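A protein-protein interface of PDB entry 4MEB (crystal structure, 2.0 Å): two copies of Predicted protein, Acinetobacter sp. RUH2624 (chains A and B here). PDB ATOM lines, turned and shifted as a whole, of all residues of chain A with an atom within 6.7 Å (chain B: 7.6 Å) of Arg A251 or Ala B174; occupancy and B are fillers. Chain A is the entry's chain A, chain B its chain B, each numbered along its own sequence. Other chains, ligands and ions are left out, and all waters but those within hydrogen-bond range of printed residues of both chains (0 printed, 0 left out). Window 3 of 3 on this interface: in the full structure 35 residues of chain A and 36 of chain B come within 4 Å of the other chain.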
ATOM      1  N   PRO A 162       1.438 -29.718 -17.346  1.00  0.00           N
ATOM      2  CA  PRO A 162       1.539 -29.009 -16.064  1.00  0.00           C
ATOM      3  C   PRO A 162       2.918 -28.405 -15.870  1.00  0.00           C
ATOM      4  O   PRO A 162       3.918 -29.109 -15.970  1.00  0.00           O
ATOM      5  CB  PRO A 162       1.296 -30.118 -15.032  1.00  0.00           C
ATOM      6  CG  PRO A 162       0.395 -31.057 -15.730  1.00  0.00           C
ATOM      7  CD  PRO A 162       0.845 -31.057 -17.181  1.00  0.00           C
ATOM      8  N   ASP A 163       2.955 -27.099 -15.638  1.00  0.00           N
ATOM      9  CA  ASP A 163       4.181 -26.404 -15.266  1.00  0.00           C
ATOM     10  C   ASP A 163       3.783 -25.162 -14.470  1.00  0.00           C
ATOM     11  O   ASP A 163       2.605 -25.022 -14.121  1.00  0.00           O
ATOM     12  CB  ASP A 163       5.075 -26.097 -16.496  1.00  0.00           C
ATOM     13  CG  ASP A 163       4.686 -24.815 -17.242  1.00  0.00           C
ATOM     14  OD1 ASP A 163       3.532 -24.350 -17.126  1.00  0.00           O
ATOM     15  OD2 ASP A 163       5.561 -24.282 -17.977  1.00  0.00           O
ATOM     16  N   PHE A 167      -0.202 -22.370 -12.507  1.00  0.00           N
ATOM     17  CA  PHE A 167      -0.502 -21.502 -11.367  1.00  0.00           C
ATOM     18  C   PHE A 167      -0.794 -20.055 -11.801  1.00  0.00           C
ATOM     19  O   PHE A 167      -0.935 -19.170 -10.945  1.00  0.00           O
ATOM     20  CB  PHE A 167       0.682 -21.455 -10.398  1.00  0.00           C
ATOM     21  CG  PHE A 167       0.927 -22.744  -9.646  1.00  0.00           C
ATOM     22  CD1 PHE A 167      -0.113 -23.620  -9.364  1.00  0.00           C
ATOM     23  CD2 PHE A 167       2.207 -23.058  -9.198  1.00  0.00           C
ATOM     24  CE1 PHE A 167       0.120 -24.796  -8.647  1.00  0.00           C
ATOM     25  CE2 PHE A 167       2.452 -24.230  -8.488  1.00  0.00           C
ATOM     26  CZ  PHE A 167       1.409 -25.102  -8.214  1.00  0.00           C
ATOM     27  N   SER A 245      -4.590 -33.081  -8.139  1.00  0.00           N
ATOM     28  CA  SER A 245      -3.185 -33.460  -8.100  1.00  0.00           C
ATOM     29  C   SER A 245      -2.296 -32.583  -8.985  1.00  0.00           C
ATOM     30  O   SER A 245      -1.089 -32.823  -9.079  1.00  0.00           O
ATOM     31  CB  SER A 245      -3.021 -34.930  -8.503  1.00  0.00           C
ATOM     32  OG  SER A 245      -3.505 -35.804  -7.495  1.00  0.00           O
ATOM     33  N   HIS A 246      -2.880 -31.570  -9.629  1.00  0.00           N
ATOM     34  CA  HIS A 246      -2.106 -30.728 -10.540  1.00  0.00           C
ATOM     35  C   HIS A 246      -0.956 -30.004  -9.848  1.00  0.00           C
ATOM     36  O   HIS A 246       0.091 -29.846 -10.441  1.00  0.00           O
ATOM     37  CB  HIS A 246      -2.981 -29.719 -11.309  1.00  0.00           C
ATOM     38  CG  HIS A 246      -3.388 -30.200 -12.667  1.00  0.00           C
ATOM     39  ND1 HIS A 246      -4.550 -29.800 -13.284  1.00  0.00           N
ATOM     40  CD2 HIS A 246      -2.790 -31.076 -13.514  1.00  0.00           C
ATOM     41  CE1 HIS A 246      -4.658 -30.411 -14.453  1.00  0.00           C
ATOM     42  NE2 HIS A 246      -3.605 -31.192 -14.616  1.00  0.00           N
ATOM     43  N   ALA A 247      -1.147 -29.561  -8.609  1.00  0.00           N
ATOM     44  CA  ALA A 247      -0.058 -28.855  -7.943  1.00  0.00           C
ATOM     45  C   ALA A 247       1.134 -29.811  -7.711  1.00  0.00           C
ATOM     46  O   ALA A 247       2.305 -29.426  -7.892  1.00  0.00           O
ATOM     47  CB  ALA A 247      -0.526 -28.207  -6.651  1.00  0.00           C
ATOM     48  N   ASP A 248       0.837 -31.058  -7.349  1.00  0.00           N
ATOM     49  CA  ASP A 248       1.878 -32.095  -7.320  1.00  0.00           C
ATOM     50  C   ASP A 248       2.526 -32.285  -8.695  1.00  0.00           C
ATOM     51  O   ASP A 248       3.755 -32.338  -8.797  1.00  0.00           O
ATOM     52  CB  ASP A 248       1.331 -33.448  -6.844  1.00  0.00           C
ATOM     53  CG  ASP A 248       1.011 -33.466  -5.363  1.00  0.00           C
ATOM     54  OD1 ASP A 248       1.520 -32.595  -4.624  1.00  0.00           O
ATOM     55  OD2 ASP A 248       0.252 -34.361  -4.943  1.00  0.00           O
ATOM     56  N   SER A 249       1.702 -32.383  -9.743  1.00  0.00           N
ATOM     57  CA  SER A 249       2.209 -32.613 -11.095  1.00  0.00           C
ATOM     58  C   SER A 249       3.121 -31.462 -11.541  1.00  0.00           C
ATOM     59  O   SER A 249       4.130 -31.671 -12.212  1.00  0.00           O
ATOM     60  CB  SER A 249       1.055 -32.810 -12.084  1.00  0.00           C
ATOM     61  OG  SER A 249       0.328 -33.997 -11.789  1.00  0.00           O
ATOM     62  N   ILE A 250       2.764 -30.246 -11.146  1.00  0.00           N
ATOM     63  CA  ILE A 250       3.573 -29.074 -11.460  1.00  0.00           C
ATOM     64  C   ILE A 250       4.935 -29.131 -10.781  1.00  0.00           C
ATOM     65  O   ILE A 250       5.974 -28.905 -11.429  1.00  0.00           O
ATOM     66  CB  ILE A 250       2.819 -27.772 -11.101  1.00  0.00           C
ATOM     67  CG1 ILE A 250       1.611 -27.606 -12.031  1.00  0.00           C
ATOM     68  CG2 ILE A 250       3.731 -26.567 -11.218  1.00  0.00           C
ATOM     69  CD1 ILE A 250       0.554 -26.652 -11.495  1.00  0.00           C
ATOM     70  N   ARG A 251       4.944 -29.441  -9.484  1.00  0.00           N
ATOM     71  CA  ARG A 251       6.198 -29.511  -8.752  1.00  0.00           C
ATOM     72  C   ARG A 251       7.098 -30.612  -9.307  1.00  0.00           C
ATOM     73  O   ARG A 251       8.310 -30.438  -9.396  1.00  0.00           O
ATOM     74  CB  ARG A 251       5.944 -29.665  -7.249  1.00  0.00           C
ATOM     75  CG  ARG A 251       5.170 -28.485  -6.659  1.00  0.00           C
ATOM     76  CD  ARG A 251       4.944 -28.615  -5.153  1.00  0.00           C
ATOM     77  NE  ARG A 251       3.865 -29.535  -4.811  1.00  0.00           N
ATOM     78  CZ  ARG A 251       2.677 -29.161  -4.339  1.00  0.00           C
ATOM     79  NH1 ARG A 251       2.401 -27.871  -4.148  1.00  0.00           N
ATOM     80  NH2 ARG A 251       1.767 -30.082  -4.046  1.00  0.00           N
ATOM     81  N   GLN A 252       6.492 -31.726  -9.697  1.00  0.00           N
ATOM     82  CA  GLN A 252       7.219 -32.845 -10.279  1.00  0.00           C
ATOM     83  C   GLN A 252       7.837 -32.499 -11.633  1.00  0.00           C
ATOM     84  O   GLN A 252       9.003 -32.826 -11.896  1.00  0.00           O
ATOM     85  CB  GLN A 252       6.290 -34.048 -10.418  1.00  0.00           C
ATOM     86  CG  GLN A 252       5.871 -34.630  -9.072  1.00  0.00           C
ATOM     87  CD  GLN A 252       4.685 -35.568  -9.195  1.00  0.00           C
ATOM     88  OE1 GLN A 252       4.092 -35.703 -10.270  1.00  0.00           O
ATOM     89  NE2 GLN A 252       4.340 -36.235  -8.095  1.00  0.00           N
ATOM     90  N   ASN A 253       7.060 -31.852 -12.496  1.00  0.00           N
ATOM     91  CA  ASN A 253       7.567 -31.492 -13.823  1.00  0.00           C
ATOM     92  C   ASN A 253       8.621 -30.392 -13.714  1.00  0.00           C
ATOM     93  O   ASN A 253       9.643 -30.420 -14.408  1.00  0.00           O
ATOM     94  CB  ASN A 253       6.430 -31.072 -14.770  1.00  0.00           C
ATOM     95  CG  ASN A 253       5.619 -32.264 -15.288  1.00  0.00           C
ATOM     96  OD1 ASN A 253       6.042 -33.413 -15.168  1.00  0.00           O
ATOM     97  ND2 ASN A 253       4.452 -31.987 -15.871  1.00  0.00           N
ATOM     98  N   GLU A 254       8.388 -29.435 -12.824  1.00  0.00           N
ATOM     99  CA  GLU A 254       9.382 -28.386 -12.602  1.00  0.00           C
ATOM    100  C   GLU A 254      10.695 -28.979 -12.067  1.00  0.00           C
ATOM    101  O   GLU A 254      11.778 -28.556 -12.474  1.00  0.00           O
ATOM    102  CB  GLU A 254       8.853 -27.277 -11.680  1.00  0.00           C
ATOM    103  CG  GLU A 254       7.726 -26.414 -12.295  1.00  0.00           C
ATOM    104  CD  GLU A 254       8.184 -25.553 -13.464  1.00  0.00           C
ATOM    105  OE1 GLU A 254       9.397 -25.267 -13.582  1.00  0.00           O
ATOM    106  OE2 GLU A 254       7.325 -25.158 -14.279  1.00  0.00           O
ATOM    107  N   ALA A 255      10.602 -29.961 -11.168  1.00  0.00           N
ATOM    108  CA  ALA A 255      11.811 -30.625 -10.665  1.00  0.00           C
ATOM    109  C   ALA A 255      12.556 -31.322 -11.802  1.00  0.00           C
ATOM    110  O   ALA A 255      13.787 -31.258 -11.892  1.00  0.00           O
ATOM    111  CB  ALA A 255      11.472 -31.615  -9.545  1.00  0.00           C
ATOM    112  N   LEU A 256      11.801 -31.981 -12.676  1.00  0.00           N
ATOM    113  CA  LEU A 256      12.384 -32.632 -13.844  1.00  0.00           C
ATOM    114  C   LEU A 256      13.129 -31.616 -14.715  1.00  0.00           C
ATOM    115  O   LEU A 256      14.302 -31.823 -15.063  1.00  0.00           O
ATOM    116  CB  LEU A 256      11.304 -33.375 -14.651  1.00  0.00           C
ATOM    117  CG  LEU A 256      10.935 -34.770 -14.095  1.00  0.00           C
ATOM    118  CD1 LEU A 256       9.633 -35.326 -14.705  1.00  0.00           C
ATOM    119  CD2 LEU A 256      12.078 -35.740 -14.331  1.00  0.00           C
ATOM    120  N   TYR B 172      -5.979 -21.427 -10.635  1.00  0.00           N
ATOM    121  CA  TYR B 172      -5.381 -22.473  -9.810  1.00  0.00           C
ATOM    122  C   TYR B 172      -4.034 -22.039  -9.232  1.00  0.00           C
ATOM    123  O   TYR B 172      -3.282 -21.286  -9.872  1.00  0.00           O
ATOM    124  CB  TYR B 172      -5.218 -23.759 -10.632  1.00  0.00           C
ATOM    125  CG  TYR B 172      -4.818 -24.991  -9.849  1.00  0.00           C
ATOM    126  CD1 TYR B 172      -5.707 -25.599  -8.962  1.00  0.00           C
ATOM    127  CD2 TYR B 172      -3.559 -25.563 -10.015  1.00  0.00           C
ATOM    128  CE1 TYR B 172      -5.349 -26.739  -8.252  1.00  0.00           C
ATOM    129  CE2 TYR B 172      -3.188 -26.703  -9.314  1.00  0.00           C
ATOM    130  CZ  TYR B 172      -4.092 -27.290  -8.432  1.00  0.00           C
ATOM    131  OH  TYR B 172      -3.733 -28.424  -7.731  1.00  0.00           O
ATOM    132  N   THR B 173      -3.738 -22.506  -8.022  1.00  0.00           N
ATOM    133  CA  THR B 173      -2.542 -22.083  -7.308  1.00  0.00           C
ATOM    134  C   THR B 173      -1.930 -23.272  -6.567  1.00  0.00           C
ATOM    135  O   THR B 173      -2.508 -24.364  -6.528  1.00  0.00           O
ATOM    136  CB  THR B 173      -2.830 -20.957  -6.269  1.00  0.00           C
ATOM    137  OG1 THR B 173      -3.436 -21.515  -5.101  1.00  0.00           O
ATOM    138  CG2 THR B 173      -3.729 -19.841  -6.830  1.00  0.00           C
ATOM    139  N   ALA B 174      -0.763 -23.056  -5.974  1.00  0.00           N
ATOM    140  CA  ALA B 174      -0.080 -24.110  -5.232  1.00  0.00           C
ATOM    141  C   ALA B 174      -0.873 -24.491  -3.988  1.00  0.00           C
ATOM    142  O   ALA B 174      -0.650 -25.541  -3.408  1.00  0.00           O
ATOM    143  CB  ALA B 174       1.338 -23.671  -4.856  1.00  0.00           C
ATOM    144  N   ASP B 175      -1.794 -23.615  -3.600  1.00  0.00           N
ATOM    145  CA  ASP B 175      -2.704 -23.847  -2.482  1.00  0.00           C
ATOM    146  C   ASP B 175      -4.063 -24.423  -2.940  1.00  0.00           C
ATOM    147  O   ASP B 175      -4.970 -24.587  -2.134  1.00  0.00           O
ATOM    148  CB  ASP B 175      -2.918 -22.528  -1.724  1.00  0.00           C
ATOM    149  CG  ASP B 175      -3.686 -22.707  -0.424  1.00  0.00           C
ATOM    150  OD1 ASP B 175      -3.493 -23.741   0.256  1.00  0.00           O
ATOM    151  OD2 ASP B 175      -4.487 -21.809  -0.086  1.00  0.00           O
ATOM    152  N   GLY B 176      -4.206 -24.733  -4.227  1.00  0.00           N
ATOM    153  CA  GLY B 176      -5.490 -25.185  -4.751  1.00  0.00           C
ATOM    154  C   GLY B 176      -6.217 -24.084  -5.509  1.00  0.00           C
ATOM    155  O   GLY B 176      -5.574 -23.144  -5.978  1.00  0.00           O
ATOM    156  N   PRO B 177      -7.555 -24.189  -5.629  1.00  0.00           N
ATOM    157  CA  PRO B 177      -8.351 -23.223  -6.407  1.00  0.00           C
ATOM    158  C   PRO B 177      -7.993 -21.777  -6.061  1.00  0.00           C
ATOM    159  O   PRO B 177      -7.850 -21.439  -4.894  1.00  0.00           O
ATOM    160  CB  PRO B 177      -9.785 -23.555  -6.000  1.00  0.00           C
ATOM    161  CG  PRO B 177      -9.736 -25.035  -5.758  1.00  0.00           C
ATOM    162  CD  PRO B 177      -8.414 -25.225  -5.021  1.00  0.00           C
ATOM    163  N   GLY B 178      -7.797 -20.956  -7.080  1.00  0.00           N
ATOM    164  CA  GLY B 178      -7.360 -19.591  -6.880  1.00  0.00           C
ATOM    165  C   GLY B 178      -8.473 -18.569  -6.987  1.00  0.00           C
ATOM    166  O   GLY B 178      -9.611 -18.886  -7.366  1.00  0.00           O
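No position is printed for both chains. Of the 6 pairs that touch across the chains among the printed residues, none has its exchanged pair printed and touching as well.
Printed residues of chain A within 4 Å of Ala B174: Phe A167 and Arg A251. Of the printed residues of chain A, Tyr B172 touches Phe A167 (3.2 Å), His A246 (3.6 Å) and Ala A247 (3.0 Å). Of the printed residues of chain B, Phe A167 touches Tyr B172 (3.2 Å), Thr B173 (3.3 Å) and Ala B174 (3.3 Å). Of the printed residues of chain A, Thr B173 touches Phe A167 (3.3 Å). Of the printed residues of chain B, His A246 touches Tyr B172. Gly B178 touches none of the printed residues of chain A.
OG1 of Thr B173 sits at hydrogen-bond distance from O of Gly B176 (2.8 Å). The backbone carbonyl oxygen of Ala A247 sits close to the guanidinium group of Arg A251 (3.5 Å). OD1 of Asp A248 is in salt-bridge range of NH2 of Arg A251 (2.6 Å). The side-chain hydroxyl of Thr B173 lies close to the backbone NH of Asp B175 (3.1 Å).
The backbone NH (N) of Ala A247 sits at hydrogen-bond distance from the side-chain hydroxyl (OH) of Tyr B172 (3.0 Å). O of Phe A167 sits close to O of Tyr B172, 3.3 Å away.
Phe A167 touches Thr B173. Phe A167 touches Ala B174. His A246 touches Tyr B172. O of Ala B174 touches NH1 of Arg A251, 3.9 Å away.
Of the 15 printed residues of chain A, 4 touch a printed residue of chain B. Printed residues of chain A that touch a printed residue of chain B: Phe A167, His A246, Ala A247 and Arg A251. Hydrophobic or aromatic side chains of chain A within 4 Å of the printed part of chain B: Phe A167, His A246 and Ala A247. Printed residues of chain B that touch a printed residue of chain A: Tyr B172, Thr B173 and Ala B174. Hydrophobic or aromatic side chains of chain B within 4 Å of the printed part of chain A: Tyr B172 and Ala B174. Among the printed residues, no Asp or Glu carboxylate lies within 4 Å of a Lys or Arg side-chain nitrogen of the other chain.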
